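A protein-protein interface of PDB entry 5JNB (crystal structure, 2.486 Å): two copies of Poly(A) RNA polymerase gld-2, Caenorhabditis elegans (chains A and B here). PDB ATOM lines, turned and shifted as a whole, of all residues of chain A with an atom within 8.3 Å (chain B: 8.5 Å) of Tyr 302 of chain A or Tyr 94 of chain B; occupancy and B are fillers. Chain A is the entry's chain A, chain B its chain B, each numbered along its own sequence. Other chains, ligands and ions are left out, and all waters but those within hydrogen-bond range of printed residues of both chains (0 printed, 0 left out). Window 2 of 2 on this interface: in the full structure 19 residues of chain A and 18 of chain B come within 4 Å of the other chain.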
ATOM      1  N   LYS A 171      11.109  16.895 -19.130  1.00  0.00           N
ATOM      2  CA  LYS A 171      12.197  16.240 -19.867  1.00  0.00           C
ATOM      3  C   LYS A 171      12.827  17.143 -20.922  1.00  0.00           C
ATOM      4  O   LYS A 171      12.145  17.752 -21.753  1.00  0.00           O
ATOM      5  CB  LYS A 171      11.715  14.939 -20.525  1.00  0.00           C
ATOM      6  CG  LYS A 171      11.405  13.847 -19.528  1.00  0.00           C
ATOM      7  CD  LYS A 171      11.033  12.527 -20.191  1.00  0.00           C
ATOM      8  CE  LYS A 171      12.249  11.807 -20.777  1.00  0.00           C
ATOM      9  NZ  LYS A 171      11.858  10.474 -21.331  1.00  0.00           N
ATOM     10  N   PHE A 174      12.069  17.706 -24.931  1.00  0.00           N
ATOM     11  CA  PHE A 174      10.705  17.224 -25.159  1.00  0.00           C
ATOM     12  C   PHE A 174       9.716  18.383 -25.104  1.00  0.00           C
ATOM     13  O   PHE A 174       8.770  18.404 -24.307  1.00  0.00           O
ATOM     14  CB  PHE A 174      10.319  16.168 -24.134  1.00  0.00           C
ATOM     15  CG  PHE A 174      10.793  14.795 -24.479  1.00  0.00           C
ATOM     16  CD1 PHE A 174      12.146  14.539 -24.667  1.00  0.00           C
ATOM     17  CD2 PHE A 174       9.888  13.749 -24.603  1.00  0.00           C
ATOM     18  CE1 PHE A 174      12.584  13.281 -24.989  1.00  0.00           C
ATOM     19  CE2 PHE A 174      10.325  12.490 -24.923  1.00  0.00           C
ATOM     20  CZ  PHE A 174      11.681  12.258 -25.117  1.00  0.00           C
ATOM     21  N   TRP A 283      13.960  16.216 -29.380  1.00  0.00           N
ATOM     22  CA  TRP A 283      14.245  14.801 -29.095  1.00  0.00           C
ATOM     23  C   TRP A 283      15.636  14.433 -29.585  1.00  0.00           C
ATOM     24  O   TRP A 283      15.935  13.264 -29.779  1.00  0.00           O
ATOM     25  CB  TRP A 283      13.206  13.873 -29.735  1.00  0.00           C
ATOM     26  CG  TRP A 283      11.752  14.304 -29.561  1.00  0.00           C
ATOM     27  CD1 TRP A 283      11.056  14.408 -28.382  1.00  0.00           C
ATOM     28  CD2 TRP A 283      10.822  14.651 -30.603  1.00  0.00           C
ATOM     29  NE1 TRP A 283       9.764  14.812 -28.630  1.00  0.00           N
ATOM     30  CE2 TRP A 283       9.591  14.954 -29.982  1.00  0.00           C
ATOM     31  CE3 TRP A 283      10.911  14.730 -31.999  1.00  0.00           C
ATOM     32  CZ2 TRP A 283       8.463  15.331 -30.706  1.00  0.00           C
ATOM     33  CZ3 TRP A 283       9.781  15.120 -32.725  1.00  0.00           C
ATOM     34  CH2 TRP A 283       8.578  15.413 -32.075  1.00  0.00           C
ATOM     35  N   ARG A 284      16.471  15.451 -29.779  1.00  0.00           N
ATOM     36  CA  ARG A 284      17.828  15.324 -30.315  1.00  0.00           C
ATOM     37  C   ARG A 284      17.923  14.798 -31.764  1.00  0.00           C
ATOM     38  O   ARG A 284      19.023  14.467 -32.205  1.00  0.00           O
ATOM     39  CB  ARG A 284      18.676  14.436 -29.401  1.00  0.00           C
ATOM     40  CG  ARG A 284      18.487  14.728 -27.927  1.00  0.00           C
ATOM     41  CD  ARG A 284      19.775  15.165 -27.267  1.00  0.00           C
ATOM     42  NE  ARG A 284      19.573  15.487 -25.854  1.00  0.00           N
ATOM     43  CZ  ARG A 284      20.560  15.721 -24.989  1.00  0.00           C
ATOM     44  NH1 ARG A 284      21.831  15.656 -25.389  1.00  0.00           N
ATOM     45  NH2 ARG A 284      20.278  16.013 -23.721  1.00  0.00           N
ATOM     46  N   HIS A 299      24.581  12.115 -33.538  1.00  0.00           N
ATOM     47  CA  HIS A 299      23.600  11.643 -32.581  1.00  0.00           C
ATOM     48  C   HIS A 299      24.218  10.652 -31.551  1.00  0.00           C
ATOM     49  O   HIS A 299      25.034   9.814 -31.933  1.00  0.00           O
ATOM     50  CB  HIS A 299      22.490  10.939 -33.430  1.00  0.00           C
ATOM     51  CG  HIS A 299      21.922  11.763 -34.559  1.00  0.00           C
ATOM     52  ND1 HIS A 299      20.568  11.962 -34.657  1.00  0.00           N
ATOM     53  CD2 HIS A 299      22.485  12.675 -35.395  1.00  0.00           C
ATOM     54  CE1 HIS A 299      20.317  12.804 -35.639  1.00  0.00           C
ATOM     55  NE2 HIS A 299      21.462  13.264 -36.100  1.00  0.00           N
ATOM     56  N   SER A 300      23.856  10.739 -30.273  1.00  0.00           N
ATOM     57  CA  SER A 300      24.303   9.732 -29.313  1.00  0.00           C
ATOM     58  C   SER A 300      23.785   8.380 -29.781  1.00  0.00           C
ATOM     59  O   SER A 300      22.751   8.315 -30.444  1.00  0.00           O
ATOM     60  CB  SER A 300      23.813  10.030 -27.908  1.00  0.00           C
ATOM     61  OG  SER A 300      23.906   8.853 -27.134  1.00  0.00           O
ATOM     62  N   ILE A 301      24.494   7.301 -29.467  1.00  0.00           N
ATOM     63  CA  ILE A 301      23.956   5.984 -29.808  1.00  0.00           C
ATOM     64  C   ILE A 301      22.704   5.656 -28.982  1.00  0.00           C
ATOM     65  O   ILE A 301      21.890   4.840 -29.400  1.00  0.00           O
ATOM     66  CB  ILE A 301      24.998   4.847 -29.655  1.00  0.00           C
ATOM     67  CG1 ILE A 301      25.638   4.825 -28.261  1.00  0.00           C
ATOM     68  CG2 ILE A 301      26.073   4.949 -30.754  1.00  0.00           C
ATOM     69  CD1 ILE A 301      26.793   3.798 -28.138  1.00  0.00           C
ATOM     70  N   TYR A 302      22.532   6.323 -27.845  1.00  0.00           N
ATOM     71  CA  TYR A 302      21.341   6.150 -27.019  1.00  0.00           C
ATOM     72  C   TYR A 302      20.147   6.983 -27.482  1.00  0.00           C
ATOM     73  O   TYR A 302      19.016   6.710 -27.091  1.00  0.00           O
ATOM     74  CB  TYR A 302      21.655   6.488 -25.565  1.00  0.00           C
ATOM     75  CG  TYR A 302      22.847   5.732 -25.025  1.00  0.00           C
ATOM     76  CD1 TYR A 302      22.725   4.412 -24.589  1.00  0.00           C
ATOM     77  CD2 TYR A 302      24.105   6.329 -24.966  1.00  0.00           C
ATOM     78  CE1 TYR A 302      23.830   3.709 -24.093  1.00  0.00           C
ATOM     79  CE2 TYR A 302      25.207   5.636 -24.467  1.00  0.00           C
ATOM     80  CZ  TYR A 302      25.064   4.327 -24.033  1.00  0.00           C
ATOM     81  OH  TYR A 302      26.169   3.647 -23.552  1.00  0.00           O
ATOM     82  N   ASP A 303      20.398   8.011 -28.286  1.00  0.00           N
ATOM     83  CA  ASP A 303      19.316   8.807 -28.866  1.00  0.00           C
ATOM     84  C   ASP A 303      18.521   7.950 -29.846  1.00  0.00           C
ATOM     85  O   ASP A 303      17.305   8.081 -29.946  1.00  0.00           O
ATOM     86  CB  ASP A 303      19.857  10.045 -29.589  1.00  0.00           C
ATOM     87  CG  ASP A 303      20.522  11.039 -28.656  1.00  0.00           C
ATOM     88  OD1 ASP A 303      20.169  11.096 -27.465  1.00  0.00           O
ATOM     89  OD2 ASP A 303      21.404  11.783 -29.120  1.00  0.00           O
ATOM     90  N   GLU A 304      19.224   7.065 -30.548  1.00  0.00           N
ATOM     91  CA  GLU A 304      18.647   6.249 -31.612  1.00  0.00           C
ATOM     92  C   GLU A 304      17.461   5.429 -31.143  1.00  0.00           C
ATOM     93  O   GLU A 304      16.474   5.275 -31.859  1.00  0.00           O
ATOM     94  CB  GLU A 304      19.705   5.319 -32.195  1.00  0.00           C
ATOM     95  N   MET A 305      17.567   4.883 -29.944  1.00  0.00           N
ATOM     96  CA  MET A 305      16.452   4.182 -29.338  1.00  0.00           C
ATOM     97  C   MET A 305      15.225   5.093 -29.276  1.00  0.00           C
ATOM     98  O   MET A 305      14.146   4.732 -29.747  1.00  0.00           O
ATOM     99  CB  MET A 305      16.831   3.694 -27.939  1.00  0.00           C
ATOM    100  N   VAL A 306      15.410   6.285 -28.711  1.00  0.00           N
ATOM    101  CA  VAL A 306      14.319   7.240 -28.498  1.00  0.00           C
ATOM    102  C   VAL A 306      13.761   7.741 -29.829  1.00  0.00           C
ATOM    103  O   VAL A 306      12.553   7.852 -29.985  1.00  0.00           O
ATOM    104  CB  VAL A 306      14.790   8.430 -27.632  1.00  0.00           C
ATOM    105  CG1 VAL A 306      13.637   9.005 -26.814  1.00  0.00           C
ATOM    106  CG2 VAL A 306      15.931   7.982 -26.700  1.00  0.00           C
ATOM    107  N   PHE A 307      14.644   8.014 -30.790  1.00  0.00           N
ATOM    108  CA  PHE A 307      14.229   8.426 -32.125  1.00  0.00           C
ATOM    109  C   PHE A 307      13.192   7.465 -32.652  1.00  0.00           C
ATOM    110  O   PHE A 307      12.140   7.871 -33.135  1.00  0.00           O
ATOM    111  CB  PHE A 307      15.395   8.450 -33.124  1.00  0.00           C
ATOM    112  CG  PHE A 307      16.478   9.472 -32.837  1.00  0.00           C
ATOM    113  CD1 PHE A 307      16.317  10.478 -31.890  1.00  0.00           C
ATOM    114  CD2 PHE A 307      17.656   9.452 -33.581  1.00  0.00           C
ATOM    115  CE1 PHE A 307      17.348  11.420 -31.671  1.00  0.00           C
ATOM    116  CE2 PHE A 307      18.663  10.373 -33.367  1.00  0.00           C
ATOM    117  CZ  PHE A 307      18.512  11.365 -32.429  1.00  0.00           C
ATOM    118  N   GLU A 308      13.507   6.174 -32.559  1.00  0.00           N
ATOM    119  CA  GLU A 308      12.684   5.123 -33.149  1.00  0.00           C
ATOM    120  C   GLU A 308      11.327   5.037 -32.482  1.00  0.00           C
ATOM    121  O   GLU A 308      10.330   4.765 -33.133  1.00  0.00           O
ATOM    122  CB  GLU A 308      13.412   3.777 -33.091  1.00  0.00           C
ATOM    123  CG  GLU A 308      14.678   3.711 -33.981  1.00  0.00           C
ATOM    124  CD  GLU A 308      14.407   4.012 -35.472  1.00  0.00           C
ATOM    125  OE1 GLU A 308      13.332   3.612 -35.981  1.00  0.00           O
ATOM    126  OE2 GLU A 308      15.278   4.630 -36.138  1.00  0.00           O
ATOM    127  N   ALA B  37      24.701   4.573 -13.531  1.00  0.00           N
ATOM    128  CA  ALA B  37      24.365   5.395 -14.693  1.00  0.00           C
ATOM    129  C   ALA B  37      25.437   6.457 -14.968  1.00  0.00           C
ATOM    130  O   ALA B  37      25.685   6.800 -16.121  1.00  0.00           O
ATOM    131  CB  ALA B  37      23.011   6.046 -14.494  1.00  0.00           C
ATOM    132  N   PRO B  40      30.094   5.514 -16.302  1.00  0.00           N
ATOM    133  CA  PRO B  40      30.809   5.613 -17.592  1.00  0.00           C
ATOM    134  C   PRO B  40      31.343   7.015 -17.928  1.00  0.00           C
ATOM    135  O   PRO B  40      32.314   7.125 -18.684  1.00  0.00           O
ATOM    136  CB  PRO B  40      29.747   5.211 -18.620  1.00  0.00           C
ATOM    137  CG  PRO B  40      28.751   4.422 -17.872  1.00  0.00           C
ATOM    138  CD  PRO B  40      28.705   5.058 -16.503  1.00  0.00           C
ATOM    139  N   VAL B  41      30.717   8.055 -17.374  1.00  0.00           N
ATOM    140  CA  VAL B  41      31.134   9.434 -17.603  1.00  0.00           C
ATOM    141  C   VAL B  41      32.174   9.905 -16.587  1.00  0.00           C
ATOM    142  O   VAL B  41      33.033  10.737 -16.894  1.00  0.00           O
ATOM    143  CB  VAL B  41      29.931  10.386 -17.556  1.00  0.00           C
ATOM    144  CG1 VAL B  41      30.397  11.791 -17.579  1.00  0.00           C
ATOM    145  CG2 VAL B  41      28.993  10.110 -18.719  1.00  0.00           C
ATOM    146  N   LEU B  87      25.888  17.771 -18.081  1.00  0.00           N
ATOM    147  CA  LEU B  87      26.369  16.532 -18.647  1.00  0.00           C
ATOM    148  C   LEU B  87      25.695  15.340 -17.950  1.00  0.00           C
ATOM    149  O   LEU B  87      25.237  14.421 -18.627  1.00  0.00           O
ATOM    150  CB  LEU B  87      27.885  16.471 -18.542  1.00  0.00           C
ATOM    151  CG  LEU B  87      28.586  15.195 -18.986  1.00  0.00           C
ATOM    152  CD1 LEU B  87      28.087  14.793 -20.365  1.00  0.00           C
ATOM    153  CD2 LEU B  87      30.094  15.430 -19.002  1.00  0.00           C
ATOM    154  N   ILE B  88      25.593  15.373 -16.617  1.00  0.00           N
ATOM    155  CA  ILE B  88      24.973  14.276 -15.856  1.00  0.00           C
ATOM    156  C   ILE B  88      23.481  14.208 -16.140  1.00  0.00           C
ATOM    157  O   ILE B  88      22.903  13.120 -16.185  1.00  0.00           O
ATOM    158  CB  ILE B  88      25.212  14.420 -14.323  1.00  0.00           C
ATOM    159  CG1 ILE B  88      26.689  14.225 -14.002  1.00  0.00           C
ATOM    160  CG2 ILE B  88      24.391  13.399 -13.499  1.00  0.00           C
ATOM    161  CD1 ILE B  88      27.024  14.655 -12.644  1.00  0.00           C
ATOM    162  N   LEU B  89      22.869  15.369 -16.358  1.00  0.00           N
ATOM    163  CA  LEU B  89      21.470  15.448 -16.772  1.00  0.00           C
ATOM    164  C   LEU B  89      21.239  14.696 -18.090  1.00  0.00           C
ATOM    165  O   LEU B  89      20.310  13.896 -18.193  1.00  0.00           O
ATOM    166  CB  LEU B  89      21.037  16.911 -16.906  1.00  0.00           C
ATOM    167  CG  LEU B  89      19.546  17.268 -16.967  1.00  0.00           C
ATOM    168  CD1 LEU B  89      19.306  18.707 -16.499  1.00  0.00           C
ATOM    169  CD2 LEU B  89      19.000  17.072 -18.370  1.00  0.00           C
ATOM    170  N   SER B  90      22.086  14.945 -19.083  1.00  0.00           N
ATOM    171  CA  SER B  90      22.018  14.226 -20.372  1.00  0.00           C
ATOM    172  C   SER B  90      22.173  12.713 -20.222  1.00  0.00           C
ATOM    173  O   SER B  90      21.467  11.943 -20.873  1.00  0.00           O
ATOM    174  CB  SER B  90      23.095  14.722 -21.335  1.00  0.00           C
ATOM    175  OG  SER B  90      23.032  16.127 -21.444  1.00  0.00           O
ATOM    176  N   THR B  91      23.115  12.290 -19.379  1.00  0.00           N
ATOM    177  CA  THR B  91      23.318  10.869 -19.153  1.00  0.00           C
ATOM    178  C   THR B  91      22.072  10.233 -18.517  1.00  0.00           C
ATOM    179  O   THR B  91      21.594   9.212 -18.992  1.00  0.00           O
ATOM    180  CB  THR B  91      24.544  10.597 -18.258  1.00  0.00           C
ATOM    181  OG1 THR B  91      25.705  11.251 -18.784  1.00  0.00           O
ATOM    182  CG2 THR B  91      24.799   9.118 -18.179  1.00  0.00           C
ATOM    183  N   LEU B  92      21.527  10.852 -17.469  1.00  0.00           N
ATOM    184  CA  LEU B  92      20.424  10.250 -16.714  1.00  0.00           C
ATOM    185  C   LEU B  92      19.074  10.231 -17.454  1.00  0.00           C
ATOM    186  O   LEU B  92      18.150   9.507 -17.077  1.00  0.00           O
ATOM    187  CB  LEU B  92      20.249  10.973 -15.384  1.00  0.00           C
ATOM    188  CG  LEU B  92      21.382  10.810 -14.373  1.00  0.00           C
ATOM    189  CD1 LEU B  92      21.095  11.623 -13.169  1.00  0.00           C
ATOM    190  CD2 LEU B  92      21.522   9.361 -13.982  1.00  0.00           C
ATOM    191  N   GLN B  93      18.963  11.023 -18.512  1.00  0.00           N
ATOM    192  CA  GLN B  93      17.711  11.150 -19.233  1.00  0.00           C
ATOM    193  C   GLN B  93      17.370   9.832 -19.919  1.00  0.00           C
ATOM    194  O   GLN B  93      16.193   9.489 -20.069  1.00  0.00           O
ATOM    195  CB  GLN B  93      17.801  12.294 -20.240  1.00  0.00           C
ATOM    196  CG  GLN B  93      18.496  11.953 -21.571  1.00  0.00           C
ATOM    197  CD  GLN B  93      18.966  13.189 -22.342  1.00  0.00           C
ATOM    198  OE1 GLN B  93      18.654  14.322 -21.965  1.00  0.00           O
ATOM    199  NE2 GLN B  93      19.735  12.976 -23.404  1.00  0.00           N
ATOM    200  N   TYR B  94      18.400   9.091 -20.322  1.00  0.00           N
ATOM    201  CA  TYR B  94      18.211   7.801 -20.982  1.00  0.00           C
ATOM    202  C   TYR B  94      17.738   6.689 -20.031  1.00  0.00           C
ATOM    203  O   TYR B  94      17.224   5.675 -20.480  1.00  0.00           O
ATOM    204  CB  TYR B  94      19.505   7.361 -21.678  1.00  0.00           C
ATOM    205  CG  TYR B  94      20.068   8.394 -22.633  1.00  0.00           C
ATOM    206  CD1 TYR B  94      19.324   8.838 -23.725  1.00  0.00           C
ATOM    207  CD2 TYR B  94      21.345   8.917 -22.452  1.00  0.00           C
ATOM    208  CE1 TYR B  94      19.827   9.789 -24.601  1.00  0.00           C
ATOM    209  CE2 TYR B  94      21.865   9.869 -23.327  1.00  0.00           C
ATOM    210  CZ  TYR B  94      21.097  10.301 -24.402  1.00  0.00           C
ATOM    211  OH  TYR B  94      21.603  11.241 -25.284  1.00  0.00           O
ATOM    212  N   GLU B  95      17.900   6.889 -18.725  1.00  0.00           N
ATOM    213  CA  GLU B  95      17.540   5.874 -17.736  1.00  0.00           C
ATOM    214  C   GLU B  95      16.031   5.778 -17.471  1.00  0.00           C
ATOM    215  O   GLU B  95      15.384   6.779 -17.188  1.00  0.00           O
ATOM    216  CB  GLU B  95      18.262   6.158 -16.413  1.00  0.00           C
ATOM    217  CG  GLU B  95      19.785   6.188 -16.515  1.00  0.00           C
ATOM    218  CD  GLU B  95      20.377   4.857 -16.980  1.00  0.00           C
ATOM    219  OE1 GLU B  95      19.885   3.796 -16.533  1.00  0.00           O
ATOM    220  OE2 GLU B  95      21.327   4.879 -17.802  1.00  0.00           O
ATOM    221  N   LYS B  96      15.482   4.570 -17.516  1.00  0.00           N
ATOM    222  CA  LYS B  96      14.048   4.358 -17.306  1.00  0.00           C
ATOM    223  C   LYS B  96      13.533   4.663 -15.891  1.00  0.00           C
ATOM    224  O   LYS B  96      12.339   4.935 -15.712  1.00  0.00           O
ATOM    225  CB  LYS B  96      13.689   2.925 -17.686  1.00  0.00           C
ATOM    226  CG  LYS B  96      13.411   2.790 -19.176  1.00  0.00           C
ATOM    227  CD  LYS B  96      14.062   1.556 -19.800  1.00  0.00           C
ATOM    228  CE  LYS B  96      15.056   1.943 -20.913  1.00  0.00           C
ATOM    229  NZ  LYS B  96      16.103   0.901 -21.145  1.00  0.00           N
ATOM    230  N   PHE B  97      14.407   4.649 -14.887  1.00  0.00           N
ATOM    231  CA  PHE B  97      13.936   4.969 -13.544  1.00  0.00           C
ATOM    232  C   PHE B  97      13.899   6.480 -13.295  1.00  0.00           C
ATOM    233  O   PHE B  97      13.263   6.954 -12.337  1.00  0.00           O
ATOM    234  CB  PHE B  97      14.784   4.257 -12.474  1.00  0.00           C
ATOM    235  CG  PHE B  97      16.255   4.590 -12.502  1.00  0.00           C
ATOM    236  CD1 PHE B  97      16.782   5.535 -11.626  1.00  0.00           C
ATOM    237  CD2 PHE B  97      17.116   3.917 -13.345  1.00  0.00           C
ATOM    238  CE1 PHE B  97      18.142   5.832 -11.612  1.00  0.00           C
ATOM    239  CE2 PHE B  97      18.482   4.214 -13.346  1.00  0.00           C
ATOM    240  CZ  PHE B  97      18.993   5.174 -12.474  1.00  0.00           C
ATOM    241  N   VAL B  98      14.551   7.244 -14.169  1.00  0.00           N
ATOM    242  CA  VAL B  98      14.534   8.690 -14.046  1.00  0.00           C
ATOM    243  C   VAL B  98      13.351   9.244 -14.835  1.00  0.00           C
ATOM    244  O   VAL B  98      13.209   8.940 -16.010  1.00  0.00           O
ATOM    245  CB  VAL B  98      15.856   9.297 -14.523  1.00  0.00           C
ATOM    246  CG1 VAL B  98      15.787  10.843 -14.578  1.00  0.00           C
ATOM    247  CG2 VAL B  98      16.981   8.812 -13.633  1.00  0.00           C
ATOM    248  N   GLN B 101      13.929  15.835 -14.489  1.00  0.00           N
ATOM    249  CA  GLN B 101      15.097  16.536 -13.963  1.00  0.00           C
ATOM    250  C   GLN B 101      15.006  18.031 -14.199  1.00  0.00           C
ATOM    251  O   GLN B 101      14.348  18.471 -15.124  1.00  0.00           O
ATOM    252  CB  GLN B 101      16.380  16.059 -14.609  1.00  0.00           C
ATOM    253  CG  GLN B 101      16.858  14.732 -14.198  1.00  0.00           C
ATOM    254  CD  GLN B 101      18.036  14.323 -15.033  1.00  0.00           C
ATOM    255  OE1 GLN B 101      19.165  14.202 -14.535  1.00  0.00           O
ATOM    256  NE2 GLN B 101      17.788  14.128 -16.322  1.00  0.00           N
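No position is printed for both chains. Of the 5 pairs that touch across the chains among the printed residues, none has its exchanged pair printed and touching as well.
Arg 284 of chain A touches Ser 90 of chain B (NH2 to OG, 3.6 Å). Tyr 94 of chain B touches Ser 300 of chain A (OH to CB, 3.6 Å). Tyr 94 of chain B touches Tyr 302 of chain A (CD1 to CB, 3.8 Å).
Ile 301 of chain A touches none of the printed residues of chain B. Tyr 302 of chain A touches just one residue of chain B: Tyr 94 (3.8 Å). Of the printed residues of chain A, Ser 90 of chain B touches Arg 284 (3.6 Å). Of the printed residues of chain A, Gln 93 of chain B touches Arg 284 (2.9 Å). Tyr 94 of chain B touches just these residues of chain A: Ser 300, Tyr 302 and Asp 303. The nearest residue of chain B that does not touch Tyr 302 of chain A is Pro 40 of chain B (6.3 Å). The nearest residue of chain A that does not touch Tyr 94 of chain B is Arg 284 of chain A (4.4 Å). The nearest printed residue of chain A that does not touch Ser 90 of chain B is Asp 303 of chain A (6.8 Å).
Of the 16 printed residues of chain B, 3 touch a printed residue of chain A. Printed residues of chain B that touch a printed residue of chain A: Ser 90, Gln 93 and Tyr 94.
The side-chain hydroxyl of Ser 300 of chain A is in hydrogen-bond range of the backbone NH of Tyr 302 of chain A (3.0 Å). The backbone NH (N) of Ser 300 of chain A sits at hydrogen-bond distance from the side-chain carboxylate (OD2) of Asp 303 of chain A, at 2.9 Å. The backbone carbonyl oxygen (O) of Ser 90 of chain B sits close to the side-chain amide nitrogen (NE2) of Gln 93 of chain B (3.2 Å). NE2 of Gln 93 of chain B lies close to OH of Tyr 94 of chain B (3.2 Å).
OE1 of Gln 93 of chain B is in hydrogen-bond range of NH2 of Arg 284 of chain A (2.9 Å). The side-chain carboxylate (OD1) of Asp 303 of chain A lies within hydrogen-bond range of the side-chain hydroxyl (OH) of Tyr 94 of chain B (2.6 Å).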
